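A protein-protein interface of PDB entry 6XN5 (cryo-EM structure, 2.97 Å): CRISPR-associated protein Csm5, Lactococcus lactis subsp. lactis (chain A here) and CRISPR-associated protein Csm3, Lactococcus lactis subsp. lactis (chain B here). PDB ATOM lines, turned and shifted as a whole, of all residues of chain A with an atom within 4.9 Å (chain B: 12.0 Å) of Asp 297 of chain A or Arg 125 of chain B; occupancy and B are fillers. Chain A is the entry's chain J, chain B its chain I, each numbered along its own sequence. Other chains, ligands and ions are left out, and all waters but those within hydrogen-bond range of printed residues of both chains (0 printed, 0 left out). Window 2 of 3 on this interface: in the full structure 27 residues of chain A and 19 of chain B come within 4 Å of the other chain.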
ATOM      1  N   LYS A 144      34.615 -11.755 -12.123  1.00  0.00           N
ATOM      2  CA  LYS A 144      33.795 -12.801 -11.503  1.00  0.00           C
ATOM      3  C   LYS A 144      33.724 -14.044 -12.396  1.00  0.00           C
ATOM      4  O   LYS A 144      32.681 -14.400 -12.946  1.00  0.00           O
ATOM      5  CB  LYS A 144      32.394 -12.278 -11.218  1.00  0.00           C
ATOM      6  CG  LYS A 144      32.305 -10.830 -10.773  1.00  0.00           C
ATOM      7  CD  LYS A 144      32.938 -10.592  -9.418  1.00  0.00           C
ATOM      8  CE  LYS A 144      32.534  -9.226  -8.887  1.00  0.00           C
ATOM      9  NZ  LYS A 144      33.180  -8.897  -7.593  1.00  0.00           N
ATOM     10  N   LEU A 281      37.624  -9.352  -3.422  1.00  0.00           N
ATOM     11  CA  LEU A 281      38.221  -9.997  -4.590  1.00  0.00           C
ATOM     12  C   LEU A 281      38.575  -9.060  -5.738  1.00  0.00           C
ATOM     13  O   LEU A 281      39.435  -9.427  -6.545  1.00  0.00           O
ATOM     14  CB  LEU A 281      37.307 -11.115  -5.121  1.00  0.00           C
ATOM     15  CG  LEU A 281      35.905 -10.891  -5.694  1.00  0.00           C
ATOM     16  CD1 LEU A 281      35.940 -10.776  -7.208  1.00  0.00           C
ATOM     17  CD2 LEU A 281      34.982 -12.027  -5.281  1.00  0.00           C
ATOM     18  N   ASN A 293      32.328   2.551  -6.362  1.00  0.00           N
ATOM     19  CA  ASN A 293      31.711   1.366  -6.954  1.00  0.00           C
ATOM     20  C   ASN A 293      31.322   0.367  -5.863  1.00  0.00           C
ATOM     21  O   ASN A 293      30.131   0.114  -5.608  1.00  0.00           O
ATOM     22  CB  ASN A 293      32.726   0.751  -7.942  1.00  0.00           C
ATOM     23  CG  ASN A 293      32.098   0.082  -9.151  1.00  0.00           C
ATOM     24  OD1 ASN A 293      31.021   0.451  -9.601  1.00  0.00           O
ATOM     25  ND2 ASN A 293      32.785  -0.920  -9.681  1.00  0.00           N
ATOM     26  N   ASP A 294      32.327  -0.121  -5.126  1.00  0.00           N
ATOM     27  CA  ASP A 294      32.019  -1.043  -4.042  1.00  0.00           C
ATOM     28  C   ASP A 294      31.360  -0.352  -2.852  1.00  0.00           C
ATOM     29  O   ASP A 294      30.757  -1.040  -2.030  1.00  0.00           O
ATOM     30  CB  ASP A 294      33.265  -1.833  -3.602  1.00  0.00           C
ATOM     31  CG  ASP A 294      34.418  -0.960  -3.094  1.00  0.00           C
ATOM     32  OD1 ASP A 294      34.276  -0.241  -2.088  1.00  0.00           O
ATOM     33  OD2 ASP A 294      35.521  -1.059  -3.667  1.00  0.00           O
ATOM     34  N   SER A 295      31.417   0.981  -2.760  1.00  0.00           N
ATOM     35  CA  SER A 295      30.713   1.670  -1.681  1.00  0.00           C
ATOM     36  C   SER A 295      29.202   1.578  -1.848  1.00  0.00           C
ATOM     37  O   SER A 295      28.488   1.295  -0.881  1.00  0.00           O
ATOM     38  CB  SER A 295      31.161   3.126  -1.590  1.00  0.00           C
ATOM     39  OG  SER A 295      32.572   3.223  -1.516  1.00  0.00           O
ATOM     40  N   PHE A 296      28.688   1.788  -3.067  1.00  0.00           N
ATOM     41  CA  PHE A 296      27.248   1.564  -3.220  1.00  0.00           C
ATOM     42  C   PHE A 296      26.918   0.072  -3.237  1.00  0.00           C
ATOM     43  O   PHE A 296      25.835  -0.317  -2.768  1.00  0.00           O
ATOM     44  CB  PHE A 296      26.642   2.308  -4.437  1.00  0.00           C
ATOM     45  CG  PHE A 296      27.291   2.037  -5.799  1.00  0.00           C
ATOM     46  CD1 PHE A 296      27.146   0.813  -6.457  1.00  0.00           C
ATOM     47  CD2 PHE A 296      27.927   3.068  -6.478  1.00  0.00           C
ATOM     48  CE1 PHE A 296      27.704   0.600  -7.705  1.00  0.00           C
ATOM     49  CE2 PHE A 296      28.478   2.860  -7.727  1.00  0.00           C
ATOM     50  CZ  PHE A 296      28.358   1.625  -8.340  1.00  0.00           C
ATOM     51  N   ASP A 297      27.858  -0.772  -3.706  1.00  0.00           N
ATOM     52  CA  ASP A 297      27.655  -2.224  -3.658  1.00  0.00           C
ATOM     53  C   ASP A 297      27.540  -2.733  -2.221  1.00  0.00           C
ATOM     54  O   ASP A 297      26.854  -3.727  -1.960  1.00  0.00           O
ATOM     55  CB  ASP A 297      28.799  -2.958  -4.370  1.00  0.00           C
ATOM     56  CG  ASP A 297      28.862  -2.673  -5.863  1.00  0.00           C
ATOM     57  OD1 ASP A 297      27.806  -2.476  -6.497  1.00  0.00           O
ATOM     58  OD2 ASP A 297      29.981  -2.657  -6.406  1.00  0.00           O
ATOM     59  N   ILE A 298      28.214  -2.072  -1.283  1.00  0.00           N
ATOM     60  CA  ILE A 298      28.106  -2.441   0.123  1.00  0.00           C
ATOM     61  C   ILE A 298      26.899  -1.761   0.766  1.00  0.00           C
ATOM     62  O   ILE A 298      26.127  -2.394   1.495  1.00  0.00           O
ATOM     63  CB  ILE A 298      29.421  -2.105   0.858  1.00  0.00           C
ATOM     64  CG1 ILE A 298      30.518  -3.098   0.472  1.00  0.00           C
ATOM     65  CG2 ILE A 298      29.248  -2.121   2.370  1.00  0.00           C
ATOM     66  CD1 ILE A 298      31.924  -2.563   0.657  1.00  0.00           C
ATOM     67  N   LEU A 299      26.682  -0.477   0.465  1.00  0.00           N
ATOM     68  CA  LEU A 299      25.695   0.304   1.200  1.00  0.00           C
ATOM     69  C   LEU A 299      24.269   0.042   0.716  1.00  0.00           C
ATOM     70  O   LEU A 299      23.319   0.553   1.319  1.00  0.00           O
ATOM     71  CB  LEU A 299      26.048   1.789   1.096  1.00  0.00           C
ATOM     72  CG  LEU A 299      25.574   2.722   2.207  1.00  0.00           C
ATOM     73  CD1 LEU A 299      26.286   2.334   3.485  1.00  0.00           C
ATOM     74  CD2 LEU A 299      25.851   4.169   1.855  1.00  0.00           C
ATOM     75  N   LYS A 300      24.089  -0.739  -0.351  1.00  0.00           N
ATOM     76  CA  LYS A 300      22.756  -1.287  -0.579  1.00  0.00           C
ATOM     77  C   LYS A 300      22.529  -2.592   0.176  1.00  0.00           C
ATOM     78  O   LYS A 300      21.497  -3.239  -0.032  1.00  0.00           O
ATOM     79  CB  LYS A 300      22.500  -1.492  -2.074  1.00  0.00           C
ATOM     80  CG  LYS A 300      21.059  -1.210  -2.509  1.00  0.00           C
ATOM     81  CD  LYS A 300      20.758   0.279  -2.527  1.00  0.00           C
ATOM     82  CE  LYS A 300      19.355   0.552  -3.042  1.00  0.00           C
ATOM     83  NZ  LYS A 300      19.218   0.230  -4.489  1.00  0.00           N
ATOM     84  N   GLN A 301      23.464  -3.002   1.038  1.00  0.00           N
ATOM     85  CA  GLN A 301      23.256  -4.141   1.924  1.00  0.00           C
ATOM     86  C   GLN A 301      23.079  -3.744   3.387  1.00  0.00           C
ATOM     87  O   GLN A 301      22.752  -4.610   4.207  1.00  0.00           O
ATOM     88  CB  GLN A 301      24.418  -5.138   1.807  1.00  0.00           C
ATOM     89  CG  GLN A 301      24.859  -5.437   0.381  1.00  0.00           C
ATOM     90  CD  GLN A 301      23.792  -6.139  -0.437  1.00  0.00           C
ATOM     91  OE1 GLN A 301      23.019  -5.500  -1.148  1.00  0.00           O
ATOM     92  NE2 GLN A 301      23.753  -7.462  -0.346  1.00  0.00           N
ATOM     93  N   ASN B 121      32.568 -22.708   6.605  1.00  0.00           N
ATOM     94  CA  ASN B 121      31.985 -21.459   6.137  1.00  0.00           C
ATOM     95  C   ASN B 121      32.461 -21.148   4.719  1.00  0.00           C
ATOM     96  O   ASN B 121      33.405 -21.747   4.205  1.00  0.00           O
ATOM     97  CB  ASN B 121      32.355 -20.307   7.071  1.00  0.00           C
ATOM     98  CG  ASN B 121      32.299 -20.694   8.534  1.00  0.00           C
ATOM     99  OD1 ASN B 121      33.270 -20.523   9.269  1.00  0.00           O
ATOM    100  ND2 ASN B 121      31.160 -21.218   8.963  1.00  0.00           N
ATOM    101  N   THR B 122      31.792 -20.190   4.082  1.00  0.00           N
ATOM    102  CA  THR B 122      32.169 -19.781   2.732  1.00  0.00           C
ATOM    103  C   THR B 122      31.872 -18.301   2.567  1.00  0.00           C
ATOM    104  O   THR B 122      30.708 -17.896   2.623  1.00  0.00           O
ATOM    105  CB  THR B 122      31.420 -20.593   1.681  1.00  0.00           C
ATOM    106  OG1 THR B 122      31.796 -21.970   1.779  1.00  0.00           O
ATOM    107  CG2 THR B 122      31.750 -20.083   0.289  1.00  0.00           C
ATOM    108  N   ILE B 123      32.904 -17.503   2.360  1.00  0.00           N
ATOM    109  CA  ILE B 123      32.748 -16.073   2.124  1.00  0.00           C
ATOM    110  C   ILE B 123      32.614 -15.835   0.627  1.00  0.00           C
ATOM    111  O   ILE B 123      33.466 -16.259  -0.161  1.00  0.00           O
ATOM    112  CB  ILE B 123      33.938 -15.290   2.709  1.00  0.00           C
ATOM    113  CG1 ILE B 123      34.072 -15.550   4.211  1.00  0.00           C
ATOM    114  CG2 ILE B 123      33.782 -13.813   2.425  1.00  0.00           C
ATOM    115  CD1 ILE B 123      32.935 -15.019   5.039  1.00  0.00           C
ATOM    116  N   ASN B 124      31.545 -15.155   0.230  1.00  0.00           N
ATOM    117  CA  ASN B 124      31.248 -14.920  -1.176  1.00  0.00           C
ATOM    118  C   ASN B 124      31.855 -13.590  -1.636  1.00  0.00           C
ATOM    119  O   ASN B 124      32.778 -13.061  -1.011  1.00  0.00           O
ATOM    120  CB  ASN B 124      29.733 -15.019  -1.425  1.00  0.00           C
ATOM    121  CG  ASN B 124      28.909 -14.023  -0.608  1.00  0.00           C
ATOM    122  OD1 ASN B 124      29.433 -13.191   0.133  1.00  0.00           O
ATOM    123  ND2 ASN B 124      27.592 -14.106  -0.763  1.00  0.00           N
ATOM    124  N   ARG B 125      31.341 -13.064  -2.753  1.00  0.00           N
ATOM    125  CA  ARG B 125      31.649 -11.778  -3.381  1.00  0.00           C
ATOM    126  C   ARG B 125      31.557 -10.628  -2.377  1.00  0.00           C
ATOM    127  O   ARG B 125      30.885 -10.768  -1.348  1.00  0.00           O
ATOM    128  CB  ARG B 125      30.670 -11.627  -4.559  1.00  0.00           C
ATOM    129  CG  ARG B 125      30.742 -10.466  -5.564  1.00  0.00           C
ATOM    130  CD  ARG B 125      29.845  -9.301  -5.172  1.00  0.00           C
ATOM    131  NE  ARG B 125      29.847  -8.224  -6.164  1.00  0.00           N
ATOM    132  CZ  ARG B 125      30.734  -7.239  -6.240  1.00  0.00           C
ATOM    133  NH1 ARG B 125      31.745  -7.184  -5.398  1.00  0.00           N
ATOM    134  NH2 ARG B 125      30.619  -6.318  -7.186  1.00  0.00           N
ATOM    135  N   LYS B 126      32.159  -9.464  -2.682  1.00  0.00           N
ATOM    136  CA  LYS B 126      32.536  -8.411  -1.721  1.00  0.00           C
ATOM    137  C   LYS B 126      31.405  -7.865  -0.829  1.00  0.00           C
ATOM    138  O   LYS B 126      31.652  -7.064   0.082  1.00  0.00           O
ATOM    139  CB  LYS B 126      33.201  -7.252  -2.480  1.00  0.00           C
ATOM    140  CG  LYS B 126      34.209  -6.416  -1.694  1.00  0.00           C
ATOM    141  CD  LYS B 126      34.709  -5.239  -2.503  1.00  0.00           C
ATOM    142  CE  LYS B 126      35.239  -4.148  -1.591  1.00  0.00           C
ATOM    143  NZ  LYS B 126      36.386  -4.571  -0.754  1.00  0.00           N
ATOM    144  N   THR B 127      30.164  -8.293  -1.081  1.00  0.00           N
ATOM    145  CA  THR B 127      29.108  -8.227  -0.075  1.00  0.00           C
ATOM    146  C   THR B 127      29.523  -8.896   1.232  1.00  0.00           C
ATOM    147  O   THR B 127      29.127  -8.435   2.310  1.00  0.00           O
ATOM    148  CB  THR B 127      27.848  -8.897  -0.615  1.00  0.00           C
ATOM    149  OG1 THR B 127      28.084 -10.303  -0.750  1.00  0.00           O
ATOM    150  CG2 THR B 127      27.494  -8.326  -1.980  1.00  0.00           C
ATOM    151  N   ALA B 128      30.292  -9.990   1.147  1.00  0.00           N
ATOM    152  CA  ALA B 128      31.046 -10.585   2.256  1.00  0.00           C
ATOM    153  C   ALA B 128      30.132 -11.072   3.380  1.00  0.00           C
ATOM    154  O   ALA B 128      30.190 -10.607   4.519  1.00  0.00           O
ATOM    155  CB  ALA B 128      32.107  -9.611   2.785  1.00  0.00           C
ATOM    156  N   VAL B 129      29.274 -12.026   3.033  1.00  0.00           N
ATOM    157  CA  VAL B 129      28.397 -12.679   3.993  1.00  0.00           C
ATOM    158  C   VAL B 129      28.764 -14.157   4.043  1.00  0.00           C
ATOM    159  O   VAL B 129      29.055 -14.775   3.011  1.00  0.00           O
ATOM    160  CB  VAL B 129      26.901 -12.447   3.652  1.00  0.00           C
ATOM    161  CG1 VAL B 129      26.530 -12.952   2.255  1.00  0.00           C
ATOM    162  CG2 VAL B 129      25.983 -13.048   4.721  1.00  0.00           C
ATOM    163  N   ALA B 130      28.838 -14.700   5.254  1.00  0.00           N
ATOM    164  CA  ALA B 130      29.169 -16.103   5.420  1.00  0.00           C
ATOM    165  C   ALA B 130      28.026 -16.983   4.927  1.00  0.00           C
ATOM    166  O   ALA B 130      26.844 -16.668   5.092  1.00  0.00           O
ATOM    167  CB  ALA B 130      29.479 -16.412   6.884  1.00  0.00           C
ATOM    168  N   ASN B 131      28.392 -18.104   4.313  1.00  0.00           N
ATOM    169  CA  ASN B 131      27.437 -19.105   3.842  1.00  0.00           C
ATOM    170  C   ASN B 131      27.771 -20.425   4.522  1.00  0.00           C
ATOM    171  O   ASN B 131      28.501 -21.255   3.969  1.00  0.00           O
ATOM    172  CB  ASN B 131      27.481 -19.240   2.319  1.00  0.00           C
ATOM    173  CG  ASN B 131      27.239 -17.923   1.608  1.00  0.00           C
ATOM    174  OD1 ASN B 131      28.122 -17.398   0.935  1.00  0.00           O
ATOM    175  ND2 ASN B 131      26.036 -17.384   1.754  1.00  0.00           N
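Among the printed residues, merely in contact across the chains: Asp 294 of chain A with Lys 126 of chain B (3.6 Å) and Leu 281 of chain A with Arg 125 of chain B (3.8 Å).
Printed residues of chain B within 4 Å of Asp 297 of chain A: Arg 125. No residue of chain B comes within 4 Å of Asn 293 of chain A. No residue of chain B comes within 4 Å of Phe 296 of chain A. No residue of chain B comes within 4 Å of Gln 301 of chain A. Printed residues of chain B within 4 Å of Lys 144 of chain A: Arg 125. Of the printed residues of chain B, Leu 281 of chain A touches Arg 125 (3.8 Å). Of the printed residues of chain A, Lys 126 of chain B touches Asp 294. Asn 121 of chain B touches none of the printed residues of chain A. The nearest printed residue of chain A that does not touch Arg 125 of chain B is Asp 294 of chain A (5.8 Å). The nearest printed residue of chain B that does not touch Lys 144 of chain A is Lys 126 of chain B (5.0 Å).
The side-chain hydroxyl of Thr 127 of chain B lies within hydrogen-bond range of the backbone carbonyl oxygen of Arg 125 of chain B (2.9 Å).
The guanidinium group (NH1) of Arg 125 of chain B lies close to the side-chain amino group (NZ) of Lys 144 of chain A. The side-chain carboxylate (OD2) of Asp 297 of chain A is in salt-bridge range of the guanidinium group (NH2) of Arg 125 of chain B (3.8 Å).
Hydrophobic or aromatic side chains of chain A that line the printed part of chain B: Leu 281. Of the 11 printed residues of chain B, 2 touch a printed residue of chain A. Among the printed residues, 4 pairs touch across the chains. Among the printed residues, Asp or Glu carboxylates within 4 Å of a Lys or Arg side-chain nitrogen of the other chain: Asp 297 of chain A with Arg 125 of chain B (3.8 Å).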
